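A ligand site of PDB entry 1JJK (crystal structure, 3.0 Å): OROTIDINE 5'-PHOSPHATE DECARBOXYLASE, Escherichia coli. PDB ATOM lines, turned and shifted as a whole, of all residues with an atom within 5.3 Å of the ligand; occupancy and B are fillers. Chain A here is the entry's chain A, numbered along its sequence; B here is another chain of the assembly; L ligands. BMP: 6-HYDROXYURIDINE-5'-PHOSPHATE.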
ATOM      1  N   ALA A  20      11.000 -11.232 -20.420  1.00  0.00           N
ATOM      2  CA  ALA A  20      11.309 -12.638 -20.558  1.00  0.00           C
ATOM      3  C   ALA A  20      11.715 -13.243 -19.213  1.00  0.00           C
ATOM      4  O   ALA A  20      12.815 -12.981 -18.715  1.00  0.00           O
ATOM      5  CB  ALA A  20      12.431 -12.815 -21.557  1.00  0.00           C
ATOM      6  N   ASP A  22      13.263 -15.808 -17.764  1.00  0.00           N
ATOM      7  CA  ASP A  22      14.123 -16.976 -17.994  1.00  0.00           C
ATOM      8  C   ASP A  22      14.964 -17.410 -16.784  1.00  0.00           C
ATOM      9  O   ASP A  22      16.182 -17.538 -16.888  1.00  0.00           O
ATOM     10  CB  ASP A  22      15.040 -16.732 -19.187  1.00  0.00           C
ATOM     11  CG  ASP A  22      14.287 -16.216 -20.396  1.00  0.00           C
ATOM     12  OD1 ASP A  22      13.058 -15.990 -20.283  1.00  0.00           O
ATOM     13  OD2 ASP A  22      14.932 -16.042 -21.453  1.00  0.00           O
ATOM     14  N   LYS A  44       6.540 -13.289 -20.272  1.00  0.00           N
ATOM     15  CA  LYS A  44       6.773 -14.267 -21.330  1.00  0.00           C
ATOM     16  C   LYS A  44       7.476 -15.525 -20.834  1.00  0.00           C
ATOM     17  O   LYS A  44       8.673 -15.499 -20.547  1.00  0.00           O
ATOM     18  CB  LYS A  44       7.607 -13.640 -22.448  1.00  0.00           C
ATOM     19  CG  LYS A  44       8.322 -14.650 -23.348  1.00  0.00           C
ATOM     20  CD  LYS A  44       9.339 -13.989 -24.284  1.00  0.00           C
ATOM     21  CE  LYS A  44      10.572 -14.884 -24.508  1.00  0.00           C
ATOM     22  NZ  LYS A  44      10.958 -15.596 -23.228  1.00  0.00           N
ATOM     23  N   ASP A  71       6.060 -18.812 -25.022  1.00  0.00           N
ATOM     24  CA  ASP A  71       7.060 -18.775 -26.082  1.00  0.00           C
ATOM     25  C   ASP A  71       7.758 -20.115 -26.203  1.00  0.00           C
ATOM     26  O   ASP A  71       8.832 -20.364 -25.623  1.00  0.00           O
ATOM     27  CB  ASP A  71       8.054 -17.627 -25.796  1.00  0.00           C
ATOM     28  CG  ASP A  71       9.340 -17.723 -26.603  1.00  0.00           C
ATOM     29  OD1 ASP A  71       9.273 -17.736 -27.849  1.00  0.00           O
ATOM     30  OD2 ASP A  71      10.433 -17.776 -25.989  1.00  0.00           O
ATOM     31  N   LYS A  73       7.793 -21.533 -29.467  1.00  0.00           N
ATOM     32  CA  LYS A  73       8.144 -21.548 -30.889  1.00  0.00           C
ATOM     33  C   LYS A  73       7.950 -22.901 -31.545  1.00  0.00           C
ATOM     34  O   LYS A  73       8.912 -23.498 -32.069  1.00  0.00           O
ATOM     35  CB  LYS A  73       9.602 -21.129 -31.097  1.00  0.00           C
ATOM     36  CG  LYS A  73       9.972 -19.787 -30.514  1.00  0.00           C
ATOM     37  CD  LYS A  73      11.421 -19.472 -30.816  1.00  0.00           C
ATOM     38  CE  LYS A  73      11.809 -18.161 -30.177  1.00  0.00           C
ATOM     39  NZ  LYS A  73      11.626 -18.200 -28.699  1.00  0.00           N
ATOM     40  N   ASN A  97       3.441 -18.774 -29.584  1.00  0.00           N
ATOM     41  CA  ASN A  97       4.507 -18.844 -30.568  1.00  0.00           C
ATOM     42  C   ASN A  97       4.509 -19.991 -31.586  1.00  0.00           C
ATOM     43  O   ASN A  97       4.093 -21.100 -31.280  1.00  0.00           O
ATOM     44  CB  ASN A  97       5.823 -18.925 -29.809  1.00  0.00           C
ATOM     45  CG  ASN A  97       6.759 -17.856 -30.192  1.00  0.00           C
ATOM     46  OD1 ASN A  97       6.910 -17.551 -31.366  1.00  0.00           O
ATOM     47  ND2 ASN A  97       7.425 -17.271 -29.212  1.00  0.00           N
ATOM     48  N   VAL A 127       7.751 -16.785 -35.493  1.00  0.00           N
ATOM     49  CA  VAL A 127       9.105 -16.297 -35.375  1.00  0.00           C
ATOM     50  C   VAL A 127       9.745 -16.355 -36.747  1.00  0.00           C
ATOM     51  O   VAL A 127       9.722 -17.396 -37.382  1.00  0.00           O
ATOM     52  CB  VAL A 127       9.924 -17.162 -34.437  1.00  0.00           C
ATOM     53  CG1 VAL A 127      11.392 -16.799 -34.541  1.00  0.00           C
ATOM     54  CG2 VAL A 127       9.435 -16.995 -33.015  1.00  0.00           C
ATOM     55  N   VAL A 129      13.342 -14.782 -38.303  1.00  0.00           N
ATOM     56  CA  VAL A 129      14.756 -15.136 -38.115  1.00  0.00           C
ATOM     57  C   VAL A 129      15.059 -14.762 -36.676  1.00  0.00           C
ATOM     58  O   VAL A 129      14.674 -13.694 -36.214  1.00  0.00           O
ATOM     59  CB  VAL A 129      15.696 -14.323 -39.049  1.00  0.00           C
ATOM     60  CG1 VAL A 129      17.103 -14.870 -38.954  1.00  0.00           C
ATOM     61  CG2 VAL A 129      15.218 -14.403 -40.482  1.00  0.00           C
ATOM     62  N   LEU A 130      15.741 -15.637 -35.942  1.00  0.00           N
ATOM     63  CA  LEU A 130      16.045 -15.347 -34.557  1.00  0.00           C
ATOM     64  C   LEU A 130      16.998 -14.151 -34.409  1.00  0.00           C
ATOM     65  O   LEU A 130      17.996 -14.056 -35.128  1.00  0.00           O
ATOM     66  CB  LEU A 130      16.620 -16.581 -33.869  1.00  0.00           C
ATOM     67  CG  LEU A 130      15.644 -17.724 -33.576  1.00  0.00           C
ATOM     68  CD1 LEU A 130      16.392 -18.878 -32.931  1.00  0.00           C
ATOM     69  CD2 LEU A 130      14.556 -17.247 -32.653  1.00  0.00           C
ATOM     70  N   THR A 131      16.675 -13.255 -33.484  1.00  0.00           N
ATOM     71  CA  THR A 131      17.494 -12.069 -33.248  1.00  0.00           C
ATOM     72  C   THR A 131      18.942 -12.375 -32.976  1.00  0.00           C
ATOM     73  O   THR A 131      19.786 -11.513 -33.141  1.00  0.00           O
ATOM     74  CB  THR A 131      17.000 -11.248 -32.073  1.00  0.00           C
ATOM     75  OG1 THR A 131      17.140 -12.022 -30.885  1.00  0.00           O
ATOM     76  CG2 THR A 131      15.554 -10.843 -32.256  1.00  0.00           C
ATOM     77  N   SER A 132      19.253 -13.591 -32.548  1.00  0.00           N
ATOM     78  CA  SER A 132      20.633 -13.922 -32.261  1.00  0.00           C
ATOM     79  C   SER A 132      21.410 -14.307 -33.517  1.00  0.00           C
ATOM     80  O   SER A 132      22.494 -14.872 -33.429  1.00  0.00           O
ATOM     81  CB  SER A 132      20.699 -15.081 -31.262  1.00  0.00           C
ATOM     82  OG  SER A 132      20.527 -16.331 -31.906  1.00  0.00           O
ATOM     83  N   VAL A 167       7.569 -12.349 -35.348  1.00  0.00           N
ATOM     84  CA  VAL A 167       8.597 -12.000 -34.370  1.00  0.00           C
ATOM     85  C   VAL A 167       9.871 -11.746 -35.135  1.00  0.00           C
ATOM     86  O   VAL A 167      10.283 -12.551 -35.961  1.00  0.00           O
ATOM     87  CB  VAL A 167       8.852 -13.099 -33.344  1.00  0.00           C
ATOM     88  CG1 VAL A 167      10.187 -12.890 -32.667  1.00  0.00           C
ATOM     89  CG2 VAL A 167       7.777 -13.074 -32.283  1.00  0.00           C
ATOM     90  N   PRO A 189      12.467  -8.789 -29.765  1.00  0.00           N
ATOM     91  CA  PRO A 189      13.311  -9.134 -28.617  1.00  0.00           C
ATOM     92  C   PRO A 189      14.684  -8.581 -29.001  1.00  0.00           C
ATOM     93  O   PRO A 189      14.794  -7.838 -29.991  1.00  0.00           O
ATOM     94  CB  PRO A 189      13.301 -10.669 -28.603  1.00  0.00           C
ATOM     95  CG  PRO A 189      12.249 -11.071 -29.651  1.00  0.00           C
ATOM     96  CD  PRO A 189      12.310  -9.957 -30.652  1.00  0.00           C
ATOM     97  N   GLY A 190      15.726  -8.949 -28.255  1.00  0.00           N
ATOM     98  CA  GLY A 190      17.049  -8.452 -28.569  1.00  0.00           C
ATOM     99  C   GLY A 190      17.070  -6.951 -28.346  1.00  0.00           C
ATOM    100  O   GLY A 190      17.461  -6.160 -29.223  1.00  0.00           O
ATOM    101  N   ILE A 191      16.618  -6.575 -27.162  1.00  0.00           N
ATOM    102  CA  ILE A 191      16.525  -5.179 -26.749  1.00  0.00           C
ATOM    103  C   ILE A 191      17.532  -4.857 -25.664  1.00  0.00           C
ATOM    104  O   ILE A 191      17.312  -5.166 -24.496  1.00  0.00           O
ATOM    105  CB  ILE A 191      15.124  -4.880 -26.217  1.00  0.00           C
ATOM    106  CG1 ILE A 191      14.093  -5.070 -27.336  1.00  0.00           C
ATOM    107  CG2 ILE A 191      15.086  -3.497 -25.612  1.00  0.00           C
ATOM    108  CD1 ILE A 191      14.334  -4.215 -28.563  1.00  0.00           C
ATOM    109  N   ARG A 192      18.629  -4.239 -26.069  1.00  0.00           N
ATOM    110  CA  ARG A 192      19.694  -3.873 -25.139  1.00  0.00           C
ATOM    111  C   ARG A 192      19.727  -2.357 -24.964  1.00  0.00           C
ATOM    112  O   ARG A 192      20.008  -1.608 -25.899  1.00  0.00           O
ATOM    113  CB  ARG A 192      21.047  -4.347 -25.670  1.00  0.00           C
ATOM    114  CG  ARG A 192      21.194  -5.856 -25.841  1.00  0.00           C
ATOM    115  CD  ARG A 192      21.523  -6.540 -24.525  1.00  0.00           C
ATOM    116  NE  ARG A 192      20.371  -7.219 -23.923  1.00  0.00           N
ATOM    117  CZ  ARG A 192      19.951  -8.432 -24.237  1.00  0.00           C
ATOM    118  NH1 ARG A 192      20.573  -9.152 -25.165  1.00  0.00           N
ATOM    119  NH2 ARG A 192      18.907  -8.947 -23.615  1.00  0.00           N
ATOM    120  N   ALA A 198      25.412  -7.556 -24.606  1.00  0.00           N
ATOM    121  CA  ALA A 198      24.621  -8.171 -25.681  1.00  0.00           C
ATOM    122  C   ALA A 198      24.564  -9.701 -25.544  1.00  0.00           C
ATOM    123  O   ALA A 198      23.486 -10.296 -25.452  1.00  0.00           O
ATOM    124  CB  ALA A 198      25.212  -7.809 -27.046  1.00  0.00           C
ATOM    125  N   GLN A 201      23.060 -12.217 -28.378  1.00  0.00           N
ATOM    126  CA  GLN A 201      22.180 -11.324 -29.109  1.00  0.00           C
ATOM    127  C   GLN A 201      22.956 -10.638 -30.231  1.00  0.00           C
ATOM    128  O   GLN A 201      24.156 -10.428 -30.101  1.00  0.00           O
ATOM    129  CB  GLN A 201      21.630 -10.287 -28.142  1.00  0.00           C
ATOM    130  CG  GLN A 201      20.186  -9.851 -28.395  1.00  0.00           C
ATOM    131  CD  GLN A 201      19.179 -10.989 -28.286  1.00  0.00           C
ATOM    132  OE1 GLN A 201      18.934 -11.708 -29.253  1.00  0.00           O
ATOM    133  NE2 GLN A 201      18.606 -11.160 -27.093  1.00  0.00           N
ATOM    134  N   VAL A 219      10.593  -7.486 -26.171  1.00  0.00           N
ATOM    135  CA  VAL A 219      10.972  -8.437 -25.142  1.00  0.00           C
ATOM    136  C   VAL A 219      12.278  -8.074 -24.488  1.00  0.00           C
ATOM    137  O   VAL A 219      13.338  -8.110 -25.124  1.00  0.00           O
ATOM    138  CB  VAL A 219      11.109  -9.867 -25.715  1.00  0.00           C
ATOM    139  CG1 VAL A 219      11.220 -10.877 -24.570  1.00  0.00           C
ATOM    140  CG2 VAL A 219       9.939 -10.185 -26.613  1.00  0.00           C
ATOM    141  N   ILE A 220      12.213  -7.708 -23.211  1.00  0.00           N
ATOM    142  CA  ILE A 220      13.422  -7.393 -22.504  1.00  0.00           C
ATOM    143  C   ILE A 220      13.686  -8.575 -21.582  1.00  0.00           C
ATOM    144  O   ILE A 220      12.862  -8.920 -20.734  1.00  0.00           O
ATOM    145  CB  ILE A 220      13.321  -6.085 -21.663  1.00  0.00           C
ATOM    146  CG1 ILE A 220      13.166  -4.877 -22.583  1.00  0.00           C
ATOM    147  CG2 ILE A 220      14.586  -5.891 -20.843  1.00  0.00           C
ATOM    148  CD1 ILE A 220      11.764  -4.663 -23.055  1.00  0.00           C
ATOM    149  N   GLY A 221      14.851  -9.198 -21.784  1.00  0.00           N
ATOM    150  CA  GLY A 221      15.216 -10.333 -20.980  1.00  0.00           C
ATOM    151  C   GLY A 221      16.120 -10.004 -19.814  1.00  0.00           C
ATOM    152  O   GLY A 221      15.674  -9.565 -18.749  1.00  0.00           O
ATOM    153  N   ARG A 222      17.410 -10.225 -20.011  1.00  0.00           N
ATOM    154  CA  ARG A 222      18.396  -9.998 -18.979  1.00  0.00           C
ATOM    155  C   ARG A 222      18.547  -8.552 -18.456  1.00  0.00           C
ATOM    156  O   ARG A 222      18.650  -8.326 -17.232  1.00  0.00           O
ATOM    157  CB  ARG A 222      19.732 -10.581 -19.467  1.00  0.00           C
ATOM    158  CG  ARG A 222      19.760 -12.112 -19.352  1.00  0.00           C
ATOM    159  CD  ARG A 222      20.746 -12.782 -20.297  1.00  0.00           C
ATOM    160  NE  ARG A 222      20.325 -12.669 -21.693  1.00  0.00           N
ATOM    161  CZ  ARG A 222      20.998 -13.230 -22.689  1.00  0.00           C
ATOM    162  NH1 ARG A 222      22.096 -13.924 -22.440  1.00  0.00           N
ATOM    163  NH2 ARG A 222      20.569 -13.077 -23.953  1.00  0.00           N
ATOM    164  N   PRO A 223      18.568  -7.554 -19.359  1.00  0.00           N
ATOM    165  CA  PRO A 223      18.699  -6.172 -18.927  1.00  0.00           C
ATOM    166  C   PRO A 223      17.907  -5.909 -17.672  1.00  0.00           C
ATOM    167  O   PRO A 223      18.374  -5.244 -16.768  1.00  0.00           O
ATOM    168  CB  PRO A 223      18.141  -5.397 -20.102  1.00  0.00           C
ATOM    169  CG  PRO A 223      18.656  -6.205 -21.256  1.00  0.00           C
ATOM    170  CD  PRO A 223      18.405  -7.636 -20.823  1.00  0.00           C
ATOM    171  N   ASP B  76      15.827 -21.742 -30.515  1.00  0.00           N
ATOM    172  CA  ASP B  76      15.857 -20.392 -29.932  1.00  0.00           C
ATOM    173  C   ASP B  76      17.238 -19.771 -30.066  1.00  0.00           C
ATOM    174  O   ASP B  76      18.077 -20.226 -30.855  1.00  0.00           O
ATOM    175  CB  ASP B  76      15.535 -20.483 -28.438  1.00  0.00           C
ATOM    176  CG  ASP B  76      14.340 -19.658 -28.047  1.00  0.00           C
ATOM    177  OD1 ASP B  76      14.242 -18.525 -28.535  1.00  0.00           O
ATOM    178  OD2 ASP B  76      13.508 -20.147 -27.244  1.00  0.00           O
ATOM    179  N   ILE B  77      17.473 -18.717 -29.283  1.00  0.00           N
ATOM    180  CA  ILE B  77      18.773 -18.059 -29.260  1.00  0.00           C
ATOM    181  C   ILE B  77      19.677 -19.003 -28.462  1.00  0.00           C
ATOM    182  O   ILE B  77      19.220 -19.700 -27.533  1.00  0.00           O
ATOM    183  CB  ILE B  77      18.730 -16.662 -28.580  1.00  0.00           C
ATOM    184  CG1 ILE B  77      18.255 -16.772 -27.136  1.00  0.00           C
ATOM    185  CG2 ILE B  77      17.809 -15.737 -29.344  1.00  0.00           C
ATOM    186  CD1 ILE B  77      18.227 -15.432 -26.415  1.00  0.00           C
ATOM    187  N   THR B  80      19.000 -19.418 -24.677  1.00  0.00           N
ATOM    188  CA  THR B  80      17.788 -20.172 -24.335  1.00  0.00           C
ATOM    189  C   THR B  80      17.980 -21.671 -24.562  1.00  0.00           C
ATOM    190  O   THR B  80      17.694 -22.495 -23.683  1.00  0.00           O
ATOM    191  CB  THR B  80      16.583 -19.703 -25.151  1.00  0.00           C
ATOM    192  OG1 THR B  80      16.343 -18.321 -24.914  1.00  0.00           O
ATOM    193  CG2 THR B  80      15.341 -20.515 -24.752  1.00  0.00           C
HETATM  194  P   BMP L   1      17.241 -11.371 -23.639  1.00  0.00           P
HETATM  195  OP1 BMP L   1      18.578 -11.426 -24.421  1.00  0.00           O
HETATM  196  OP2 BMP L   1      16.522 -10.044 -23.700  1.00  0.00           O
HETATM  197  OP3 BMP L   1      17.489 -11.769 -22.186  1.00  0.00           O
HETATM  198  O5' BMP L   1      16.347 -12.496 -24.359  1.00  0.00           O
HETATM  199  C5' BMP L   1      15.002 -12.694 -23.863  1.00  0.00           C
HETATM  200  C4' BMP L   1      14.179 -13.760 -24.461  1.00  0.00           C
HETATM  201  O4' BMP L   1      13.686 -13.427 -25.897  1.00  0.00           O
HETATM  202  C3' BMP L   1      14.593 -15.224 -24.458  1.00  0.00           C
HETATM  203  O3' BMP L   1      13.500 -16.044 -23.886  1.00  0.00           O
HETATM  204  C2' BMP L   1      14.728 -15.591 -25.967  1.00  0.00           C
HETATM  205  O2' BMP L   1      14.598 -16.911 -26.314  1.00  0.00           O
HETATM  206  C1' BMP L   1      13.688 -14.688 -26.607  1.00  0.00           C
HETATM  207  N1  BMP L   1      13.852 -14.470 -28.133  1.00  0.00           N
HETATM  208  C2  BMP L   1      15.033 -13.880 -28.606  1.00  0.00           C
HETATM  209  O2  BMP L   1      16.012 -13.489 -27.792  1.00  0.00           O
HETATM  210  N3  BMP L   1      15.141 -13.704 -29.986  1.00  0.00           N
HETATM  211  C4  BMP L   1      14.136 -14.100 -30.844  1.00  0.00           C
HETATM  212  O4  BMP L   1      14.285 -13.925 -32.068  1.00  0.00           O
HETATM  213  C5  BMP L   1      12.967 -14.702 -30.302  1.00  0.00           C
HETATM  214  C6  BMP L   1      12.921 -14.845 -28.937  1.00  0.00           C
HETATM  215  O1  BMP L   1      11.785 -15.418 -28.422  1.00  0.00           O
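Merely in contact with the ligand: Ala 20 (3.5 Å), Leu 130 (3.4 Å), Pro 189 (3.6 Å), Val 219 (3.8 Å), Ile 220 (3.8 Å) and Ile 77 of chain B (3.3 Å). Hydrophobic or aromatic side chains within 4 Å of the ligand: Ala 20, Leu 130, Pro 189, Val 219 and Ile 77 of chain B. 17 residues have an atom within 4 Å of the ligand: Ala 20, Asp 22, Lys 44, Asp 71, Lys 73, Leu 130, Thr 131, Pro 189, Arg 192, Gln 201, Val 219, Ile 220, Gly 221, Arg 222, Asp 76 of chain B, Ile 77 of chain B and Thr 80 of chain B. The nearest printed residue that does not touch the ligand is Val 167 (4.1 Å).
The side-chain carboxylate (OD2) of Asp 71 lies within salt-bridge range of the side-chain amino group (NZ) of Lys 44 (3.6 Å). The side-chain carboxylate (OD1) of Asp 22 lies within salt-bridge range of the side-chain amino group (NZ) of Lys 44, at 3.6 Å. The backbone carbonyl oxygen (O) of Ile 220 sits at hydrogen-bond distance from the backbone NH (N) of Ala 20, 3.0 Å away. The side-chain amide nitrogen of Gln 201 sits close to the guanidinium group of Arg 192 (3.4 Å). O of Ala 198 is in hydrogen-bond range of NH1 of Arg 192. OD1 of Asp 76 of chain B lies within salt-bridge range of NZ of Lys 73 (2.6 Å). NZ of Lys 73 lies within salt-bridge range of OD1 of Asp 71, at 2.5 Å. OE1 of Gln 201 is in hydrogen-bond range of OG1 of Thr 131 (2.4 Å).
The side-chain carboxylate of Asp 76 of chain B lies within hydrogen-bond range of an oxygen (O2') of the ligand. O3' of the ligand lies within hydrogen-bond range of NZ of Lys 44. The side-chain carboxylate (OD1) of Asp 71 lies within hydrogen-bond range of an oxygen (O1) of the ligand (3.5 Å). N of Gly 221 sits at hydrogen-bond distance from OP2 of the ligand, at 2.7 Å. The side-chain hydroxyl of Thr 80 of chain B is in hydrogen-bond range of an oxygen (O2') of the ligand, 2.6 Å away. The guanidinium group of Arg 192 is in salt-bridge range of an oxygen (OP2) of the ligand (2.6 Å). An oxygen (OP1) of the ligand is in salt-bridge range of the guanidinium group (NH2) of Arg 222 (2.6 Å). An oxygen (O1) of the ligand sits at hydrogen-bond distance from the side-chain amino group (NZ) of Lys 73 (2.8 Å). N of Thr 131 is in hydrogen-bond range of O4 of the ligand (2.9 Å). NE2 of Gln 201 lies within hydrogen-bond range of OP1 of the ligand. The backbone NH (N) of Arg 222 sits at hydrogen-bond distance from an oxygen (OP3) of the ligand (2.7 Å). OG1 of Thr 131 is in hydrogen-bond range of N3 of the ligand (2.8 Å). An oxygen (O3') of the ligand is in hydrogen-bond range of the side-chain carboxylate (OD2) of Asp 22 (2.8 Å).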
